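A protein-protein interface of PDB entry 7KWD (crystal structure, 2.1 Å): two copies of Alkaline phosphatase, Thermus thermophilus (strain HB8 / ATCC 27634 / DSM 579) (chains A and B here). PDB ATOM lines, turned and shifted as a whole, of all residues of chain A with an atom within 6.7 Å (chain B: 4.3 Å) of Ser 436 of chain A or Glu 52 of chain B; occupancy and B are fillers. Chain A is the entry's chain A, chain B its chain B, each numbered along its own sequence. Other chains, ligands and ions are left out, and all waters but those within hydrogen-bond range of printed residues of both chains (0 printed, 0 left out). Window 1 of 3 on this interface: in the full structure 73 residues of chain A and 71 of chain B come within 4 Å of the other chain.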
ATOM      1  N   SER A  50       9.083 -27.234  25.217  1.00  0.00           N
ATOM      2  CA  SER A  50       7.940 -26.534  25.793  1.00  0.00           C
ATOM      3  C   SER A  50       8.080 -26.436  27.298  1.00  0.00           C
ATOM      4  O   SER A  50       8.959 -27.061  27.904  1.00  0.00           O
ATOM      5  CB  SER A  50       6.646 -27.273  25.437  1.00  0.00           C
ATOM      6  OG  SER A  50       6.525 -28.414  26.229  1.00  0.00           O
ATOM      7  N   TRP A  51       7.185 -25.644  27.907  1.00  0.00           N
ATOM      8  CA  TRP A  51       7.152 -25.541  29.362  1.00  0.00           C
ATOM      9  C   TRP A  51       6.585 -26.800  29.991  1.00  0.00           C
ATOM     10  O   TRP A  51       6.858 -27.075  31.172  1.00  0.00           O
ATOM     11  CB  TRP A  51       6.354 -24.294  29.789  1.00  0.00           C
ATOM     12  CG  TRP A  51       7.094 -22.998  29.430  1.00  0.00           C
ATOM     13  CD1 TRP A  51       6.698 -22.026  28.543  1.00  0.00           C
ATOM     14  CD2 TRP A  51       8.358 -22.565  29.959  1.00  0.00           C
ATOM     15  NE1 TRP A  51       7.655 -21.028  28.483  1.00  0.00           N
ATOM     16  CE2 TRP A  51       8.673 -21.340  29.352  1.00  0.00           C
ATOM     17  CE3 TRP A  51       9.248 -23.100  30.902  1.00  0.00           C
ATOM     18  CZ2 TRP A  51       9.840 -20.639  29.659  1.00  0.00           C
ATOM     19  CZ3 TRP A  51      10.403 -22.394  31.209  1.00  0.00           C
ATOM     20  CH2 TRP A  51      10.682 -21.177  30.586  1.00  0.00           C
ATOM     21  N   GLU A  52       5.833 -27.605  29.247  1.00  0.00           N
ATOM     22  CA  GLU A  52       5.448 -28.894  29.806  1.00  0.00           C
ATOM     23  C   GLU A  52       6.663 -29.804  29.902  1.00  0.00           C
ATOM     24  O   GLU A  52       6.852 -30.464  30.923  1.00  0.00           O
ATOM     25  CB  GLU A  52       4.345 -29.559  28.990  1.00  0.00           C
ATOM     26  CG  GLU A  52       3.068 -28.742  28.855  1.00  0.00           C
ATOM     27  CD  GLU A  52       2.324 -28.497  30.175  1.00  0.00           C
ATOM     28  OE1 GLU A  52       1.465 -27.598  30.187  1.00  0.00           O
ATOM     29  OE2 GLU A  52       2.599 -29.185  31.190  1.00  0.00           O
ATOM     30  N   ILE A  83       9.936 -15.741  24.166  1.00  0.00           N
ATOM     31  CA  ILE A  83       9.867 -15.293  22.785  1.00  0.00           C
ATOM     32  C   ILE A  83       8.573 -15.758  22.130  1.00  0.00           C
ATOM     33  O   ILE A  83       8.133 -16.895  22.323  1.00  0.00           O
ATOM     34  CB  ILE A  83      11.074 -15.749  21.953  1.00  0.00           C
ATOM     35  CG1 ILE A  83      11.316 -17.248  22.116  1.00  0.00           C
ATOM     36  CG2 ILE A  83      12.333 -14.936  22.310  1.00  0.00           C
ATOM     37  CD1 ILE A  83      12.209 -17.759  21.025  1.00  0.00           C
ATOM     38  N   ASN A  84       7.998 -14.878  21.300  1.00  0.00           N
ATOM     39  CA  ASN A  84       6.974 -15.276  20.336  1.00  0.00           C
ATOM     40  C   ASN A  84       7.642 -15.957  19.142  1.00  0.00           C
ATOM     41  O   ASN A  84       8.686 -15.509  18.649  1.00  0.00           O
ATOM     42  CB  ASN A  84       6.161 -14.057  19.883  1.00  0.00           C
ATOM     43  CG  ASN A  84       4.990 -13.769  20.796  1.00  0.00           C
ATOM     44  OD1 ASN A  84       4.357 -14.684  21.346  1.00  0.00           O
ATOM     45  ND2 ASN A  84       4.687 -12.493  20.976  1.00  0.00           N
ATOM     46  N   THR A  85       7.046 -17.066  18.688  1.00  0.00           N
ATOM     47  CA  THR A  85       7.685 -17.907  17.686  1.00  0.00           C
ATOM     48  C   THR A  85       6.986 -17.884  16.337  1.00  0.00           C
ATOM     49  O   THR A  85       7.439 -18.564  15.409  1.00  0.00           O
ATOM     50  CB  THR A  85       7.731 -19.346  18.178  1.00  0.00           C
ATOM     51  OG1 THR A  85       6.375 -19.781  18.438  1.00  0.00           O
ATOM     52  CG2 THR A  85       8.547 -19.430  19.438  1.00  0.00           C
ATOM     53  N   TYR A  91       0.865 -18.662  12.630  1.00  0.00           N
ATOM     54  CA  TYR A  91       1.076 -18.599  14.068  1.00  0.00           C
ATOM     55  C   TYR A  91       1.781 -19.809  14.625  1.00  0.00           C
ATOM     56  O   TYR A  91       2.108 -19.796  15.807  1.00  0.00           O
ATOM     57  CB  TYR A  91      -0.254 -18.399  14.756  1.00  0.00           C
ATOM     58  CG  TYR A  91      -0.568 -16.959  14.650  1.00  0.00           C
ATOM     59  CD1 TYR A  91       0.052 -16.093  15.479  1.00  0.00           C
ATOM     60  CD2 TYR A  91      -1.376 -16.446  13.657  1.00  0.00           C
ATOM     61  CE1 TYR A  91      -0.146 -14.815  15.402  1.00  0.00           C
ATOM     62  CE2 TYR A  91      -1.580 -15.110  13.579  1.00  0.00           C
ATOM     63  CZ  TYR A  91      -0.947 -14.300  14.480  1.00  0.00           C
ATOM     64  OH  TYR A  91      -1.038 -12.906  14.530  1.00  0.00           O
ATOM     65  N   VAL A  92       2.079 -20.813  13.808  1.00  0.00           N
ATOM     66  CA  VAL A  92       2.922 -21.920  14.222  1.00  0.00           C
ATOM     67  C   VAL A  92       4.076 -22.041  13.247  1.00  0.00           C
ATOM     68  O   VAL A  92       3.870 -22.331  12.056  1.00  0.00           O
ATOM     69  CB  VAL A  92       2.143 -23.234  14.300  1.00  0.00           C
ATOM     70  CG1 VAL A  92       3.070 -24.378  14.751  1.00  0.00           C
ATOM     71  CG2 VAL A  92       0.938 -23.061  15.215  1.00  0.00           C
ATOM     72  N   HIS A 318      10.704 -23.129  19.469  1.00  0.00           N
ATOM     73  CA  HIS A 318       9.247 -23.196  19.520  1.00  0.00           C
ATOM     74  C   HIS A 318       8.904 -24.405  20.390  1.00  0.00           C
ATOM     75  O   HIS A 318       9.749 -25.281  20.629  1.00  0.00           O
ATOM     76  CB  HIS A 318       8.599 -23.391  18.145  1.00  0.00           C
ATOM     77  CG  HIS A 318       9.184 -24.550  17.427  1.00  0.00           C
ATOM     78  ND1 HIS A 318       8.824 -25.853  17.709  1.00  0.00           N
ATOM     79  CD2 HIS A 318      10.190 -24.620  16.538  1.00  0.00           C
ATOM     80  CE1 HIS A 318       9.556 -26.671  16.989  1.00  0.00           C
ATOM     81  NE2 HIS A 318      10.376 -25.944  16.259  1.00  0.00           N
ATOM     82  N   ALA A 319       7.651 -24.464  20.807  1.00  0.00           N
ATOM     83  CA  ALA A 319       7.130 -25.610  21.512  1.00  0.00           C
ATOM     84  C   ALA A 319       6.633 -26.660  20.520  1.00  0.00           C
ATOM     85  O   ALA A 319       6.233 -26.343  19.394  1.00  0.00           O
ATOM     86  CB  ALA A 319       5.986 -25.194  22.439  1.00  0.00           C
ATOM     87  N   THR A 320       6.646 -27.921  20.964  1.00  0.00           N
ATOM     88  CA  THR A 320       6.156 -29.026  20.149  1.00  0.00           C
ATOM     89  C   THR A 320       5.411 -30.023  21.020  1.00  0.00           C
ATOM     90  O   THR A 320       5.890 -30.411  22.095  1.00  0.00           O
ATOM     91  CB  THR A 320       7.299 -29.715  19.407  1.00  0.00           C
ATOM     92  OG1 THR A 320       7.883 -28.761  18.547  1.00  0.00           O
ATOM     93  CG2 THR A 320       6.779 -30.919  18.570  1.00  0.00           C
ATOM     94  N   GLY A 321       4.254 -30.449  20.524  1.00  0.00           N
ATOM     95  CA  GLY A 321       3.406 -31.385  21.214  1.00  0.00           C
ATOM     96  C   GLY A 321       2.087 -30.750  21.591  1.00  0.00           C
ATOM     97  O   GLY A 321       1.218 -30.597  20.734  1.00  0.00           O
ATOM     98  N   VAL A 322       1.907 -30.343  22.852  1.00  0.00           N
ATOM     99  CA  VAL A 322       2.912 -30.407  23.885  1.00  0.00           C
ATOM    100  C   VAL A 322       2.547 -31.531  24.831  1.00  0.00           C
ATOM    101  O   VAL A 322       1.355 -31.865  24.973  1.00  0.00           O
ATOM    102  CB  VAL A 322       3.028 -29.059  24.643  1.00  0.00           C
ATOM    103  CG1 VAL A 322       3.559 -27.966  23.707  1.00  0.00           C
ATOM    104  CG2 VAL A 322       1.723 -28.650  25.273  1.00  0.00           C
ATOM    105  N   SER A 429      -1.049 -32.483  23.072  1.00  0.00           N
ATOM    106  CA  SER A 429      -2.001 -31.688  22.307  1.00  0.00           C
ATOM    107  C   SER A 429      -2.042 -32.149  20.846  1.00  0.00           C
ATOM    108  O   SER A 429      -3.073 -32.047  20.184  1.00  0.00           O
ATOM    109  CB  SER A 429      -1.644 -30.198  22.331  1.00  0.00           C
ATOM    110  OG  SER A 429      -1.242 -29.723  23.596  1.00  0.00           O
ATOM    111  N   THR A 434       3.506 -26.147  18.335  1.00  0.00           N
ATOM    112  CA  THR A 434       2.433 -25.298  18.837  1.00  0.00           C
ATOM    113  C   THR A 434       2.909 -23.852  18.879  1.00  0.00           C
ATOM    114  O   THR A 434       4.080 -23.545  18.643  1.00  0.00           O
ATOM    115  CB  THR A 434       1.952 -25.742  20.224  1.00  0.00           C
ATOM    116  OG1 THR A 434       3.006 -25.536  21.183  1.00  0.00           O
ATOM    117  CG2 THR A 434       1.536 -27.226  20.229  1.00  0.00           C
ATOM    118  N   ALA A 435       1.970 -22.960  19.174  1.00  0.00           N
ATOM    119  CA  ALA A 435       2.164 -21.520  19.055  1.00  0.00           C
ATOM    120  C   ALA A 435       2.622 -20.851  20.349  1.00  0.00           C
ATOM    121  O   ALA A 435       2.850 -19.632  20.369  1.00  0.00           O
ATOM    122  CB  ALA A 435       0.856 -20.856  18.632  1.00  0.00           C
ATOM    123  N   SER A 436       2.740 -21.601  21.413  1.00  0.00           N
ATOM    124  CA  SER A 436       3.109 -21.057  22.715  1.00  0.00           C
ATOM    125  C   SER A 436       4.402 -20.234  22.656  1.00  0.00           C
ATOM    126  O   SER A 436       5.396 -20.664  22.047  1.00  0.00           O
ATOM    127  CB  SER A 436       3.302 -22.230  23.693  1.00  0.00           C
ATOM    128  OG  SER A 436       3.990 -21.789  24.856  1.00  0.00           O
ATOM    129  N   PRO A 437       4.485 -19.132  23.378  1.00  0.00           N
ATOM    130  CA  PRO A 437       5.806 -18.520  23.599  1.00  0.00           C
ATOM    131  C   PRO A 437       6.679 -19.434  24.453  1.00  0.00           C
ATOM    132  O   PRO A 437       6.182 -20.230  25.253  1.00  0.00           O
ATOM    133  CB  PRO A 437       5.483 -17.205  24.310  1.00  0.00           C
ATOM    134  CG  PRO A 437       4.103 -17.373  24.852  1.00  0.00           C
ATOM    135  CD  PRO A 437       3.393 -18.340  23.957  1.00  0.00           C
ATOM    136  N   VAL A 438       7.995 -19.350  24.250  1.00  0.00           N
ATOM    137  CA  VAL A 438       8.921 -20.301  24.854  1.00  0.00           C
ATOM    138  C   VAL A 438      10.133 -19.574  25.439  1.00  0.00           C
ATOM    139  O   VAL A 438      10.281 -18.357  25.339  1.00  0.00           O
ATOM    140  CB  VAL A 438       9.373 -21.375  23.841  1.00  0.00           C
ATOM    141  CG1 VAL A 438       8.183 -22.264  23.506  1.00  0.00           C
ATOM    142  CG2 VAL A 438       9.934 -20.695  22.602  1.00  0.00           C
ATOM    143  N   SER B  50      -2.774 -21.108  30.529  1.00  0.00           N
ATOM    144  CA  SER B  50      -1.536 -21.648  30.021  1.00  0.00           C
ATOM    145  C   SER B  50      -0.959 -20.713  28.957  1.00  0.00           C
ATOM    146  O   SER B  50      -1.600 -19.783  28.481  1.00  0.00           O
ATOM    147  CB  SER B  50      -1.766 -23.047  29.426  1.00  0.00           C
ATOM    148  OG  SER B  50      -2.376 -22.966  28.124  1.00  0.00           O
ATOM    149  N   TRP B  51       0.283 -20.998  28.561  1.00  0.00           N
ATOM    150  CA  TRP B  51       0.912 -20.223  27.507  1.00  0.00           C
ATOM    151  C   TRP B  51       0.348 -20.547  26.134  1.00  0.00           C
ATOM    152  O   TRP B  51       0.570 -19.771  25.191  1.00  0.00           O
ATOM    153  CB  TRP B  51       2.417 -20.465  27.566  1.00  0.00           C
ATOM    154  CG  TRP B  51       3.030 -19.793  28.754  1.00  0.00           C
ATOM    155  CD1 TRP B  51       3.657 -20.392  29.812  1.00  0.00           C
ATOM    156  CD2 TRP B  51       3.056 -18.381  29.010  1.00  0.00           C
ATOM    157  NE1 TRP B  51       4.072 -19.430  30.714  1.00  0.00           N
ATOM    158  CE2 TRP B  51       3.709 -18.192  30.242  1.00  0.00           C
ATOM    159  CE3 TRP B  51       2.567 -17.265  28.329  1.00  0.00           C
ATOM    160  CZ2 TRP B  51       3.886 -16.923  30.798  1.00  0.00           C
ATOM    161  CZ3 TRP B  51       2.754 -16.006  28.874  1.00  0.00           C
ATOM    162  CH2 TRP B  51       3.405 -15.840  30.098  1.00  0.00           C
ATOM    163  N   GLU B  52      -0.311 -21.707  25.983  1.00  0.00           N
ATOM    164  CA  GLU B  52      -1.016 -21.998  24.741  1.00  0.00           C
ATOM    165  C   GLU B  52      -2.285 -21.163  24.648  1.00  0.00           C
ATOM    166  O   GLU B  52      -2.610 -20.636  23.577  1.00  0.00           O
ATOM    167  CB  GLU B  52      -1.348 -23.483  24.664  1.00  0.00           C
ATOM    168  CG  GLU B  52      -0.190 -24.430  24.781  1.00  0.00           C
ATOM    169  CD  GLU B  52       0.751 -24.389  23.577  1.00  0.00           C
ATOM    170  OE1 GLU B  52       1.799 -25.051  23.639  1.00  0.00           O
ATOM    171  OE2 GLU B  52       0.454 -23.673  22.602  1.00  0.00           O
ATOM    172  N   ASP B  53      -3.018 -21.030  25.773  1.00  0.00           N
ATOM    173  CA  ASP B  53      -4.146 -20.101  25.780  1.00  0.00           C
ATOM    174  C   ASP B  53      -3.679 -18.723  25.364  1.00  0.00           C
ATOM    175  O   ASP B  53      -4.326 -18.029  24.566  1.00  0.00           O
ATOM    176  CB  ASP B  53      -4.807 -20.001  27.159  1.00  0.00           C
ATOM    177  CG  ASP B  53      -5.232 -21.349  27.733  1.00  0.00           C
ATOM    178  OD1 ASP B  53      -5.481 -22.322  26.975  1.00  0.00           O
ATOM    179  OD2 ASP B  53      -5.330 -21.410  28.971  1.00  0.00           O
ATOM    180  N   TYR B  54      -2.552 -18.301  25.930  1.00  0.00           N
ATOM    181  CA  TYR B  54      -2.072 -16.962  25.680  1.00  0.00           C
ATOM    182  C   TYR B  54      -1.787 -16.761  24.192  1.00  0.00           C
ATOM    183  O   TYR B  54      -2.166 -15.740  23.610  1.00  0.00           O
ATOM    184  CB  TYR B  54      -0.818 -16.681  26.487  1.00  0.00           C
ATOM    185  CG  TYR B  54      -0.231 -15.375  26.030  1.00  0.00           C
ATOM    186  CD1 TYR B  54      -0.775 -14.191  26.462  1.00  0.00           C
ATOM    187  CD2 TYR B  54       0.818 -15.324  25.091  1.00  0.00           C
ATOM    188  CE1 TYR B  54      -0.283 -12.988  26.052  1.00  0.00           C
ATOM    189  CE2 TYR B  54       1.305 -14.131  24.660  1.00  0.00           C
ATOM    190  CZ  TYR B  54       0.729 -12.951  25.122  1.00  0.00           C
ATOM    191  OH  TYR B  54       1.162 -11.705  24.695  1.00  0.00           O
ATOM    192  N   ALA B  55      -1.095 -17.714  23.567  1.00  0.00           N
ATOM    193  CA  ALA B  55      -0.745 -17.557  22.158  1.00  0.00           C
ATOM    194  C   ALA B  55      -1.996 -17.434  21.295  1.00  0.00           C
ATOM    195  O   ALA B  55      -2.063 -16.591  20.397  1.00  0.00           O
ATOM    196  CB  ALA B  55       0.108 -18.741  21.698  1.00  0.00           C
ATOM    197  N   ILE B  56      -3.016 -18.247  21.578  1.00  0.00           N
ATOM    198  CA  ILE B  56      -4.252 -18.175  20.791  1.00  0.00           C
ATOM    199  C   ILE B  56      -4.891 -16.799  20.927  1.00  0.00           C
ATOM    200  O   ILE B  56      -5.258 -16.168  19.934  1.00  0.00           O
ATOM    201  CB  ILE B  56      -5.217 -19.307  21.200  1.00  0.00           C
ATOM    202  CG1 ILE B  56      -4.692 -20.610  20.617  1.00  0.00           C
ATOM    203  CG2 ILE B  56      -6.630 -18.994  20.700  1.00  0.00           C
ATOM    204  CD1 ILE B  56      -5.125 -21.862  21.368  1.00  0.00           C
ATOM    205  N   VAL B 322      -3.328 -28.972  28.083  1.00  0.00           N
ATOM    206  CA  VAL B 322      -3.475 -27.637  27.546  1.00  0.00           C
ATOM    207  C   VAL B 322      -3.875 -27.592  26.073  1.00  0.00           C
ATOM    208  O   VAL B 322      -3.525 -28.493  25.297  1.00  0.00           O
ATOM    209  CB  VAL B 322      -2.138 -26.809  27.686  1.00  0.00           C
ATOM    210  CG1 VAL B 322      -1.801 -26.590  29.137  1.00  0.00           C
ATOM    211  CG2 VAL B 322      -0.998 -27.510  26.939  1.00  0.00           C
ATOM    212  N   GLY B 323      -4.546 -26.508  25.690  1.00  0.00           N
ATOM    213  CA  GLY B 323      -5.098 -26.373  24.355  1.00  0.00           C
ATOM    214  C   GLY B 323      -4.225 -25.562  23.415  1.00  0.00           C
ATOM    215  O   GLY B 323      -4.295 -24.329  23.386  1.00  0.00           O
ATOM    216  N   GLY B 324      -3.395 -26.261  22.633  1.00  0.00           N
ATOM    217  CA  GLY B 324      -2.406 -25.624  21.774  1.00  0.00           C
ATOM    218  C   GLY B 324      -2.845 -25.597  20.318  1.00  0.00           C
ATOM    219  O   GLY B 324      -3.297 -26.613  19.770  1.00  0.00           O
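Ser 436 of chain A touches three residues of chain B. Glu 52 of chain B touches just these residues of chain A: Val 322 (3.4 Å), Thr 434 (2.8 Å), Ala 435 (3.8 Å) and Ser 436 (3.2 Å). Printed residues of chain A within 4 Å of Ala 55 of chain B: Ala 435 (3.2 Å) and Ser 436 (3.9 Å). Of the printed residues of chain A, Val 322 of chain B touches Glu 52, Val 322 and Ser 429. Of the printed residues of chain B, Ser 429 of chain A touches Val 322 (3.1 Å). Of the printed residues of chain B, Glu 52 of chain A touches Val 322. The nearest printed residue of chain B that does not touch Ser 436 of chain A is Ser 50 of chain B (6.5 Å). The nearest residue of chain A that does not touch Glu 52 of chain B is Ala 319 of chain A (4.4 Å).
The side-chain hydroxyl of Ser 50 of chain A sits close to the backbone NH of Glu 52 of chain A, at 3.2 Å. The backbone carbonyl oxygen of Ala 319 of chain A sits at hydrogen-bond distance from the backbone NH of Thr 434 of chain A (2.9 Å). The backbone NH (N) of Ser 429 of chain A lies within hydrogen-bond range of the backbone carbonyl oxygen (O) of Val 322 of chain A, 3.1 Å away. The backbone NH (N) of Glu 52 of chain B lies close to the side-chain hydroxyl (OG) of Ser 50 of chain B (3.2 Å).
Among the printed residues, merely in contact across the chains: Ala 435 of chain A with Ala 55 of chain B, Val 322 of chain A with Val 322 of chain B, Pro 437 of chain A with Trp 51 of chain B, Ser 436 of chain A with Trp 51 of chain B, Val 322 of chain A with Glu 52 of chain B, Glu 52 of chain A with Val 322 of chain B, Trp 51 of chain A with Trp 51 of chain B, Ala 435 of chain A with Glu 52 of chain B, Pro 437 of chain A with Tyr 54 of chain B and Ser 436 of chain A with Ala 55 of chain B.
Trp 51 of chain A touches its own counterpart, Trp 51 of chain B. Glu 52 of chain A touches Val 322 of chain B, and with the chains exchanged Val 322 of chain A touches Glu 52 of chain B. Val 322 of chain A touches its own counterpart, Val 322 of chain B. Positions printed for both chains: 50, 51, 52 and 322.
The side-chain hydroxyl (OG) of Ser 429 of chain A sits at hydrogen-bond distance from the backbone carbonyl oxygen (O) of Val 322 of chain B. OG1 of Thr 434 of chain A is in hydrogen-bond range of OE1 of Glu 52 of chain B (2.8 Å). The backbone NH (N) of Ser 436 of chain A sits at hydrogen-bond distance from the side-chain carboxylate (OE2) of Glu 52 of chain B, at 3.3 Å.
Printed residues of chain B that touch a printed residue of chain A: Trp 51, Glu 52, Tyr 54, Ala 55 and Val 322. Hydrophobic or aromatic side chains of chain B within 4 Å of the printed part of chain A: Trp 51, Tyr 54, Ala 55 and Val 322. Among the printed residues, 13 pairs touch across the chains. Among the printed residues, no Asp or Glu carboxylate lies within 4 Å of a Lys or Arg side-chain nitrogen of the other chain.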
